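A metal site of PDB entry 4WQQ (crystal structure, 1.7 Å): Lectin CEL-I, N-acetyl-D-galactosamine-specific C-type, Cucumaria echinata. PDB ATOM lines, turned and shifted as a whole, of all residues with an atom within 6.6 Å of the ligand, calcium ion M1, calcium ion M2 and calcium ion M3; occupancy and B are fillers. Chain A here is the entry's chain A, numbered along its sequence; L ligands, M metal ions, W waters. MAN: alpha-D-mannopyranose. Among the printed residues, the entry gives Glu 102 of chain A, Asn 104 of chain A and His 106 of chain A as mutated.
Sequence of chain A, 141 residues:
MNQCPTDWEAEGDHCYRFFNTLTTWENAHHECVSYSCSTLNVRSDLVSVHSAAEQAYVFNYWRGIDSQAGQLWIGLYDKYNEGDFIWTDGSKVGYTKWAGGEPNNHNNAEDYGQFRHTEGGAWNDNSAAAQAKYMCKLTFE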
ATOM      1  N   ASP A  78      17.928   2.803  -5.649  1.00  0.00           N
ATOM      2  CA  ASP A  78      16.686   2.126  -5.255  1.00  0.00           C
ATOM      3  C   ASP A  78      16.838   1.224  -4.018  1.00  0.00           C
ATOM      4  O   ASP A  78      16.229   0.159  -3.917  1.00  0.00           O
ATOM      5  CB  ASP A  78      16.114   1.343  -6.441  1.00  0.00           C
ATOM      6  CG  ASP A  78      16.891   0.042  -6.764  1.00  0.00           C
ATOM      7  OD1 ASP A  78      18.092  -0.059  -6.547  1.00  0.00           O
ATOM      8  OD2 ASP A  78      16.300  -0.897  -7.288  1.00  0.00           O
ATOM      9  N   LYS A  79      17.695   1.666  -3.105  1.00  0.00           N
ATOM     10  CA  LYS A  79      17.888   1.061  -1.813  1.00  0.00           C
ATOM     11  C   LYS A  79      16.575   0.883  -1.045  1.00  0.00           C
ATOM     12  O   LYS A  79      16.355  -0.154  -0.475  1.00  0.00           O
ATOM     13  CB  LYS A  79      18.842   1.901  -0.943  1.00  0.00           C
ATOM     14  CG  LYS A  79      19.071   1.309   0.410  1.00  0.00           C
ATOM     15  CD  LYS A  79      20.051   2.078   1.302  1.00  0.00           C
ATOM     16  CE  LYS A  79      19.865   1.529   2.729  1.00  0.00           C
ATOM     17  NZ  LYS A  79      21.078   1.765   3.527  1.00  0.00           N
ATOM     18  N   ASN A  81      13.250   1.232  -2.075  1.00  0.00           N
ATOM     19  CA  ASN A  81      12.203   0.625  -2.826  1.00  0.00           C
ATOM     20  C   ASN A  81      12.782   0.054  -4.082  1.00  0.00           C
ATOM     21  O   ASN A  81      12.932   0.753  -5.080  1.00  0.00           O
ATOM     22  CB  ASN A  81      11.075   1.596  -3.128  1.00  0.00           C
ATOM     23  CG  ASN A  81      10.183   1.815  -1.928  1.00  0.00           C
ATOM     24  OD1 ASN A  81       9.228   1.029  -1.680  1.00  0.00           O
ATOM     25  ND2 ASN A  81      10.513   2.789  -1.152  1.00  0.00           N
ATOM     26  N   GLU A  82      13.205  -1.210  -3.991  1.00  0.00           N
ATOM     27  CA  GLU A  82      13.769  -1.905  -5.132  1.00  0.00           C
ATOM     28  C   GLU A  82      12.952  -1.750  -6.388  1.00  0.00           C
ATOM     29  O   GLU A  82      11.746  -2.068  -6.412  1.00  0.00           O
ATOM     30  CB  GLU A  82      13.990  -3.389  -4.809  1.00  0.00           C
ATOM     31  CG  GLU A  82      14.525  -4.296  -5.931  1.00  0.00           C
ATOM     32  CD  GLU A  82      15.893  -3.873  -6.429  1.00  0.00           C
ATOM     33  OE1 GLU A  82      16.064  -3.857  -7.677  1.00  0.00           O
ATOM     34  OE2 GLU A  82      16.723  -3.511  -5.573  1.00  0.00           O
ATOM     35  N   GLY A  83      13.610  -1.339  -7.471  1.00  0.00           N
ATOM     36  CA  GLY A  83      12.939  -1.152  -8.761  1.00  0.00           C
ATOM     37  C   GLY A  83      12.338   0.222  -8.907  1.00  0.00           C
ATOM     38  O   GLY A  83      12.006   0.611 -10.043  1.00  0.00           O
ATOM     39  N   PHE A  85      13.541   3.759  -8.533  1.00  0.00           N
ATOM     40  CA  PHE A  85      14.686   4.643  -8.313  1.00  0.00           C
ATOM     41  C   PHE A  85      14.227   6.020  -7.915  1.00  0.00           C
ATOM     42  O   PHE A  85      13.216   6.490  -8.417  1.00  0.00           O
ATOM     43  CB  PHE A  85      15.585   4.672  -9.557  1.00  0.00           C
ATOM     44  CG  PHE A  85      16.470   3.424  -9.675  1.00  0.00           C
ATOM     45  CD1 PHE A  85      15.994   2.273 -10.240  1.00  0.00           C
ATOM     46  CD2 PHE A  85      17.763   3.389  -9.143  1.00  0.00           C
ATOM     47  CE1 PHE A  85      16.782   1.125 -10.311  1.00  0.00           C
ATOM     48  CE2 PHE A  85      18.549   2.275  -9.210  1.00  0.00           C
ATOM     49  CZ  PHE A  85      18.033   1.105  -9.774  1.00  0.00           C
ATOM     50  N   GLY A 101      18.697  -3.062 -21.519  1.00  0.00           N
ATOM     51  CA  GLY A 101      18.603  -4.050 -20.439  1.00  0.00           C
ATOM     52  C   GLY A 101      18.813  -3.621 -19.003  1.00  0.00           C
ATOM     53  O   GLY A 101      18.726  -4.454 -18.078  1.00  0.00           O
ATOM     54  N   GLU A 102      19.010  -2.305 -18.802  1.00  0.00           N
ATOM     55  CA  GLU A 102      19.115  -1.771 -17.440  1.00  0.00           C
ATOM     56  C   GLU A 102      17.778  -1.080 -17.064  1.00  0.00           C
ATOM     57  O   GLU A 102      17.063  -0.606 -17.996  1.00  0.00           O
ATOM     58  CB  GLU A 102      20.262  -0.766 -17.423  1.00  0.00           C
ATOM     59  CG  GLU A 102      21.547  -1.357 -17.962  1.00  0.00           C
ATOM     60  CD  GLU A 102      22.154  -2.523 -17.150  1.00  0.00           C
ATOM     61  OE1 GLU A 102      21.736  -2.726 -15.998  1.00  0.00           O
ATOM     62  OE2 GLU A 102      23.085  -3.245 -17.659  1.00  0.00           O
ATOM     63  N   PRO A 103      17.478  -0.951 -15.767  1.00  0.00           N
ATOM     64  CA  PRO A 103      18.312  -1.471 -14.629  1.00  0.00           C
ATOM     65  C   PRO A 103      18.063  -2.965 -14.484  1.00  0.00           C
ATOM     66  O   PRO A 103      16.948  -3.400 -14.671  1.00  0.00           O
ATOM     67  CB  PRO A 103      17.743  -0.737 -13.411  1.00  0.00           C
ATOM     68  CG  PRO A 103      16.362  -0.393 -13.773  1.00  0.00           C
ATOM     69  CD  PRO A 103      16.327  -0.198 -15.269  1.00  0.00           C
ATOM     70  N   ASN A 104      19.071  -3.765 -14.284  1.00  0.00           N
ATOM     71  CA  ASN A 104      18.854  -5.189 -14.195  1.00  0.00           C
ATOM     72  C   ASN A 104      19.068  -5.775 -12.826  1.00  0.00           C
ATOM     73  O   ASN A 104      18.969  -6.970 -12.679  1.00  0.00           O
ATOM     74  CB  ASN A 104      19.716  -5.894 -15.219  1.00  0.00           C
ATOM     75  CG  ASN A 104      21.203  -5.783 -14.961  1.00  0.00           C
ATOM     76  OD1 ASN A 104      21.657  -5.038 -14.115  1.00  0.00           O
ATOM     77  ND2 ASN A 104      21.974  -6.500 -15.724  1.00  0.00           N
ATOM     78  N   ASN A 105      19.403  -4.965 -11.816  1.00  0.00           N
ATOM     79  CA  ASN A 105      19.578  -5.451 -10.435  1.00  0.00           C
ATOM     80  C   ASN A 105      20.442  -6.713 -10.418  1.00  0.00           C
ATOM     81  O   ASN A 105      20.124  -7.709  -9.759  1.00  0.00           O
ATOM     82  CB  ASN A 105      18.210  -5.669  -9.762  1.00  0.00           C
ATOM     83  CG  ASN A 105      18.309  -5.707  -8.275  1.00  0.00           C
ATOM     84  OD1 ASN A 105      19.006  -4.889  -7.600  1.00  0.00           O
ATOM     85  ND2 ASN A 105      17.609  -6.662  -7.691  1.00  0.00           N
ATOM     86  N   HIS A 106      21.565  -6.646 -11.130  1.00  0.00           N
ATOM     87  CA  HIS A 106      22.312  -7.871 -11.423  1.00  0.00           C
ATOM     88  C   HIS A 106      22.699  -8.575 -10.138  1.00  0.00           C
ATOM     89  O   HIS A 106      23.019  -7.960  -9.106  1.00  0.00           O
ATOM     90  CB  HIS A 106      23.563  -7.547 -12.228  1.00  0.00           C
ATOM     91  CG  HIS A 106      24.349  -8.749 -12.608  1.00  0.00           C
ATOM     92  ND1 HIS A 106      23.975  -9.548 -13.654  1.00  0.00           N
ATOM     93  CD2 HIS A 106      25.497  -9.257 -12.119  1.00  0.00           C
ATOM     94  CE1 HIS A 106      24.864 -10.514 -13.812  1.00  0.00           C
ATOM     95  NE2 HIS A 106      25.779 -10.377 -12.867  1.00  0.00           N
ATOM     96  N   ASN A 108      20.862  -9.663  -7.971  1.00  0.00           N
ATOM     97  CA  ASN A 108      20.022  -9.156  -6.935  1.00  0.00           C
ATOM     98  C   ASN A 108      20.631  -8.120  -6.019  1.00  0.00           C
ATOM     99  O   ASN A 108      20.194  -8.020  -4.887  1.00  0.00           O
ATOM    100  CB  ASN A 108      19.478 -10.278  -6.016  1.00  0.00           C
ATOM    101  CG  ASN A 108      18.538 -11.174  -6.733  1.00  0.00           C
ATOM    102  OD1 ASN A 108      17.323 -11.043  -6.619  1.00  0.00           O
ATOM    103  ND2 ASN A 108      19.072 -12.094  -7.480  1.00  0.00           N
ATOM    104  N   ALA A 109      21.604  -7.336  -6.496  1.00  0.00           N
ATOM    105  CA  ALA A 109      22.437  -6.500  -5.663  1.00  0.00           C
ATOM    106  C   ALA A 109      22.977  -5.288  -6.377  1.00  0.00           C
ATOM    107  O   ALA A 109      24.172  -5.063  -6.372  1.00  0.00           O
ATOM    108  CB  ALA A 109      23.611  -7.311  -5.142  1.00  0.00           C
ATOM    109  N   GLU A 110      22.121  -4.568  -7.079  1.00  0.00           N
ATOM    110  CA  GLU A 110      22.550  -3.355  -7.733  1.00  0.00           C
ATOM    111  C   GLU A 110      21.515  -2.298  -7.468  1.00  0.00           C
ATOM    112  O   GLU A 110      20.412  -2.281  -8.075  1.00  0.00           O
ATOM    113  CB  GLU A 110      22.794  -3.554  -9.238  1.00  0.00           C
ATOM    114  CG  GLU A 110      23.950  -4.488  -9.573  1.00  0.00           C
ATOM    115  CD  GLU A 110      24.331  -4.423 -11.041  1.00  0.00           C
ATOM    116  OE1 GLU A 110      23.382  -4.372 -11.883  1.00  0.00           O
ATOM    117  OE2 GLU A 110      25.554  -4.468 -11.370  1.00  0.00           O
ATOM    118  N   ASP A 111      21.899  -1.357  -6.594  1.00  0.00           N
ATOM    119  CA  ASP A 111      21.000  -0.316  -6.198  1.00  0.00           C
ATOM    120  C   ASP A 111      21.428   1.131  -6.565  1.00  0.00           C
ATOM    121  O   ASP A 111      20.819   2.074  -6.133  1.00  0.00           O
ATOM    122  CB  ASP A 111      20.672  -0.428  -4.705  1.00  0.00           C
ATOM    123  CG  ASP A 111      19.819  -1.697  -4.335  1.00  0.00           C
ATOM    124  OD1 ASP A 111      19.343  -2.491  -5.222  1.00  0.00           O
ATOM    125  OD2 ASP A 111      19.610  -1.881  -3.099  1.00  0.00           O
ATOM    126  N   TYR A 112      22.491   1.300  -7.325  1.00  0.00           N
ATOM    127  CA  TYR A 112      23.182   2.601  -7.444  1.00  0.00           C
ATOM    128  C   TYR A 112      23.393   2.959  -8.892  1.00  0.00           C
ATOM    129  O   TYR A 112      24.018   2.208  -9.652  1.00  0.00           O
ATOM    130  CB  TYR A 112      24.501   2.634  -6.596  1.00  0.00           C
ATOM    131  CG  TYR A 112      24.188   2.264  -5.210  1.00  0.00           C
ATOM    132  CD1 TYR A 112      23.518   3.174  -4.377  1.00  0.00           C
ATOM    133  CD2 TYR A 112      24.347   0.938  -4.765  1.00  0.00           C
ATOM    134  CE1 TYR A 112      23.102   2.819  -3.122  1.00  0.00           C
ATOM    135  CE2 TYR A 112      23.922   0.577  -3.491  1.00  0.00           C
ATOM    136  CZ  TYR A 112      23.328   1.523  -2.682  1.00  0.00           C
ATOM    137  OH  TYR A 112      22.899   1.122  -1.402  1.00  0.00           O
ATOM    138  N   GLN A 114      24.573   5.075 -12.393  1.00  0.00           N
ATOM    139  CA  GLN A 114      25.785   5.634 -12.923  1.00  0.00           C
ATOM    140  C   GLN A 114      25.635   5.802 -14.461  1.00  0.00           C
ATOM    141  O   GLN A 114      24.915   5.027 -15.099  1.00  0.00           O
ATOM    142  CB  GLN A 114      27.017   4.734 -12.602  1.00  0.00           C
ATOM    143  CG  GLN A 114      26.904   3.310 -13.151  1.00  0.00           C
ATOM    144  CD  GLN A 114      28.011   2.340 -12.792  1.00  0.00           C
ATOM    145  OE1 GLN A 114      28.032   1.300 -13.402  1.00  0.00           O
ATOM    146  NE2 GLN A 114      28.841   2.596 -11.789  1.00  0.00           N
ATOM    147  N   ARG A 116      27.326   5.116 -18.038  1.00  0.00           N
ATOM    148  CA  ARG A 116      28.384   4.528 -18.862  1.00  0.00           C
ATOM    149  C   ARG A 116      29.141   5.607 -19.643  1.00  0.00           C
ATOM    150  O   ARG A 116      28.638   6.699 -19.844  1.00  0.00           O
ATOM    151  CB  ARG A 116      27.722   3.555 -19.881  1.00  0.00           C
ATOM    152  CG  ARG A 116      26.930   2.538 -19.134  1.00  0.00           C
ATOM    153  CD  ARG A 116      26.782   1.233 -19.812  1.00  0.00           C
ATOM    154  NE  ARG A 116      27.439   0.244 -18.953  1.00  0.00           N
ATOM    155  CZ  ARG A 116      26.891  -0.902 -18.520  1.00  0.00           C
ATOM    156  NH1 ARG A 116      25.616  -1.314 -18.857  1.00  0.00           N
ATOM    157  NH2 ARG A 116      27.635  -1.661 -17.729  1.00  0.00           N
ATOM    158  N   ASN A 124      23.391   2.766 -16.035  1.00  0.00           N
ATOM    159  CA  ASN A 124      23.423   1.439 -15.491  1.00  0.00           C
ATOM    160  C   ASN A 124      23.230   1.516 -13.958  1.00  0.00           C
ATOM    161  O   ASN A 124      23.621   2.511 -13.327  1.00  0.00           O
ATOM    162  CB  ASN A 124      24.771   0.856 -15.777  1.00  0.00           C
ATOM    163  CG  ASN A 124      24.936  -0.515 -15.205  1.00  0.00           C
ATOM    164  OD1 ASN A 124      24.060  -1.375 -15.290  1.00  0.00           O
ATOM    165  ND2 ASN A 124      26.074  -0.721 -14.551  1.00  0.00           N
ATOM    166  N   ASP A 125      22.613   0.489 -13.388  1.00  0.00           N
ATOM    167  CA  ASP A 125      22.637   0.239 -11.971  1.00  0.00           C
ATOM    168  C   ASP A 125      23.839  -0.648 -11.618  1.00  0.00           C
ATOM    169  O   ASP A 125      24.160  -1.630 -12.325  1.00  0.00           O
ATOM    170  CB  ASP A 125      21.305  -0.311 -11.438  1.00  0.00           C
ATOM    171  CG  ASP A 125      20.896  -1.661 -12.084  1.00  0.00           C
ATOM    172  OD1 ASP A 125      21.386  -2.052 -13.188  1.00  0.00           O
ATOM    173  OD2 ASP A 125      20.033  -2.295 -11.505  1.00  0.00           O
ATOM    174  N   ASN A 126      24.454  -0.330 -10.493  1.00  0.00           N
ATOM    175  CA  ASN A 126      25.598  -1.107 -10.072  1.00  0.00           C
ATOM    176  C   ASN A 126      25.546  -1.279  -8.534  1.00  0.00           C
ATOM    177  O   ASN A 126      24.646  -0.767  -7.838  1.00  0.00           O
ATOM    178  CB  ASN A 126      26.891  -0.458 -10.593  1.00  0.00           C
ATOM    179  CG  ASN A 126      27.983  -1.478 -10.954  1.00  0.00           C
ATOM    180  OD1 ASN A 126      28.141  -2.511 -10.286  1.00  0.00           O
ATOM    181  ND2 ASN A 126      28.774  -1.185 -12.014  1.00  0.00           N
ATOM    182  N   SER A 127      26.514  -1.998  -8.009  1.00  0.00           N
ATOM    183  CA  SER A 127      26.456  -2.425  -6.639  1.00  0.00           C
ATOM    184  C   SER A 127      27.114  -1.464  -5.650  1.00  0.00           C
ATOM    185  O   SER A 127      27.798  -0.562  -6.027  1.00  0.00           O
ATOM    186  CB  SER A 127      27.163  -3.766  -6.540  1.00  0.00           C
ATOM    187  OG  SER A 127      28.575  -3.526  -6.596  1.00  0.00           O
ATOM    188  N   ALA A 130      30.978  -1.566  -6.178  1.00  0.00           N
ATOM    189  CA  ALA A 130      31.511  -1.004  -7.392  1.00  0.00           C
ATOM    190  C   ALA A 130      32.101   0.380  -7.142  1.00  0.00           C
ATOM    191  O   ALA A 130      31.802   1.048  -6.136  1.00  0.00           O
ATOM    192  CB  ALA A 130      30.390  -0.928  -8.410  1.00  0.00           C
HETATM  193  C1  MAN L   1      27.564  -5.840 -16.796  1.00  0.00           C
HETATM  194  C2  MAN L   1      26.081  -5.599 -16.883  1.00  0.00           C
HETATM  195  C3  MAN L   1      25.618  -4.469 -15.971  1.00  0.00           C
HETATM  196  C4  MAN L   1      26.239  -4.653 -14.602  1.00  0.00           C
HETATM  197  C5  MAN L   1      27.779  -4.573 -14.779  1.00  0.00           C
HETATM  198  C6  MAN L   1      28.619  -4.631 -13.534  1.00  0.00           C
HETATM  199  O1  MAN L   1      28.101  -4.766 -17.528  1.00  0.00           O
HETATM  200  O2  MAN L   1      25.531  -6.805 -16.407  1.00  0.00           O
HETATM  201  O3  MAN L   1      24.198  -4.575 -15.868  1.00  0.00           O
HETATM  202  O4  MAN L   1      25.726  -3.618 -13.784  1.00  0.00           O
HETATM  203  O5  MAN L   1      28.120  -5.826 -15.472  1.00  0.00           O
HETATM  204  O6  MAN L   1      28.065  -5.784 -12.942  1.00  0.00           O
HETATM  205 CA    CA M   1      23.212  -3.190 -13.997  1.00  0.00          CA
HETATM  206 CA    CA M   2      18.190  -2.465  -7.327  1.00  0.00          CA
HETATM  207 CA    CA M   3      18.104  -3.774  -3.597  1.00  0.00          CA
HETATM  208  O   HOH W   1      27.337  -5.766  -9.884  1.00  0.00           O
HETATM  209  O   HOH W   2      18.907  -5.594  -5.051  1.00  0.00           O
HETATM  210  O   HOH W   3      18.059  -2.268  -9.663  1.00  0.00           O
HETATM  211  O   HOH W   4      16.500  -2.363  -2.789  1.00  0.00           O
HETATM  212  O   HOH W   5      30.079  -4.326 -10.424  1.00  0.00           O
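The nearest printed residue that does not touch calcium ion M1 is Asn 126 (4.7 Å).
Of the 24 residues printed, 2 come within 4 Å of calcium ion M3.
The backbone carbonyl oxygen (O) of Gln 114 sits at hydrogen-bond distance from the backbone NH (N) of Asn 124, 2.9 Å away.
The side-chain carboxylate (OE1) of Glu 110 sits close to the backbone NH (N) of His 106, at 3.0 Å.
N of Asp 111 sits at hydrogen-bond distance from O of Asn 126 (3.1 Å).
The side-chain carboxylate of Glu 110 lies close to the side-chain amide oxygen of Asn 126, 3.4 Å away.
The side-chain carboxylate of Glu 102 lies within salt-bridge range of the guanidinium group of Arg 116 (3.4 Å).
The side-chain carboxylate of Asp 125 sits at hydrogen-bond distance from the backbone NH of Asn 105 (2.8 Å).
The side-chain carboxylate of Asp 78 lies close to the backbone NH of Gly 83 (2.7 Å).
OD1 of Asn 104 lies close to N of His 106 (3.4 Å).
Within 4 Å of calcium ion M2: Asp 78, Glu 82, Asn 105, Glu 110 and Asp 111.
Water W2 bridges the backbone carbonyl oxygen of Asn 108 and the side-chain amide nitrogen of Asn 105.
Water W1 lies within hydrogen-bond range of the side-chain carboxylate of Glu 110 (2.7 Å), an oxygen (O6) of the ligand (3.1 Å) and the side-chain amide oxygen of Asn 126 (3.4 Å).
Merely in contact with the ligand: Asn 126.
Within 4 Å of the ligand: Glu 102, Asn 104, Glu 110, Arg 116, Asn 124, Asp 125 and Asn 126.
Calcium ion M1 is bound by OD1 of Asp 125 (2.3 Å), OD1 of Asn 124 (2.4 Å), OD1 of Asn 104 (2.4 Å), OE1 of Glu 110 (2.4 Å), O of Asp 125 (2.5 Å), O3 of the ligand (2.5 Å), OE1 of Glu 102 (2.5 Å) and O4 of the ligand (2.6 Å).
The guanidinium group (NH2) of Arg 116 is in hydrogen-bond range of an oxygen (O1) of the ligand (3.1 Å).
Calcium ion M2 is bound by water W3 (2.3 Å).
O of Glu 110 binds calcium ion M2, at 2.4 Å.
The side-chain carboxylate (OD1) of Asp 111 is bound to calcium ion M2 (2.4 Å).
Calcium ion M2 is bound by the side-chain carboxylate (OD2) of Asp 78 (2.5 Å).
Calcium ion M2 is bound by the side-chain carboxylate (OE2) of Glu 82 (2.5 Å).
Calcium ion M2 is bound by OD1 of Asp 78 (2.5 Å).
Calcium ion M2 is bound by OE1 of Glu 82 (2.6 Å).
Calcium ion M2 is bound by OD1 of Asn 105, 2.6 Å away.
Calcium ion M2 has eight donor atoms within binding distance.
Calcium ion M3 is bound by water W4 (2.3 Å), the side-chain carboxylate (OD1) of Asp 111 (2.4 Å), the side-chain carboxylate (OE2) of Glu 82 (2.4 Å), water W2 (2.5 Å) and the side-chain carboxylate (OD2) of Asp 111 (2.5 Å).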
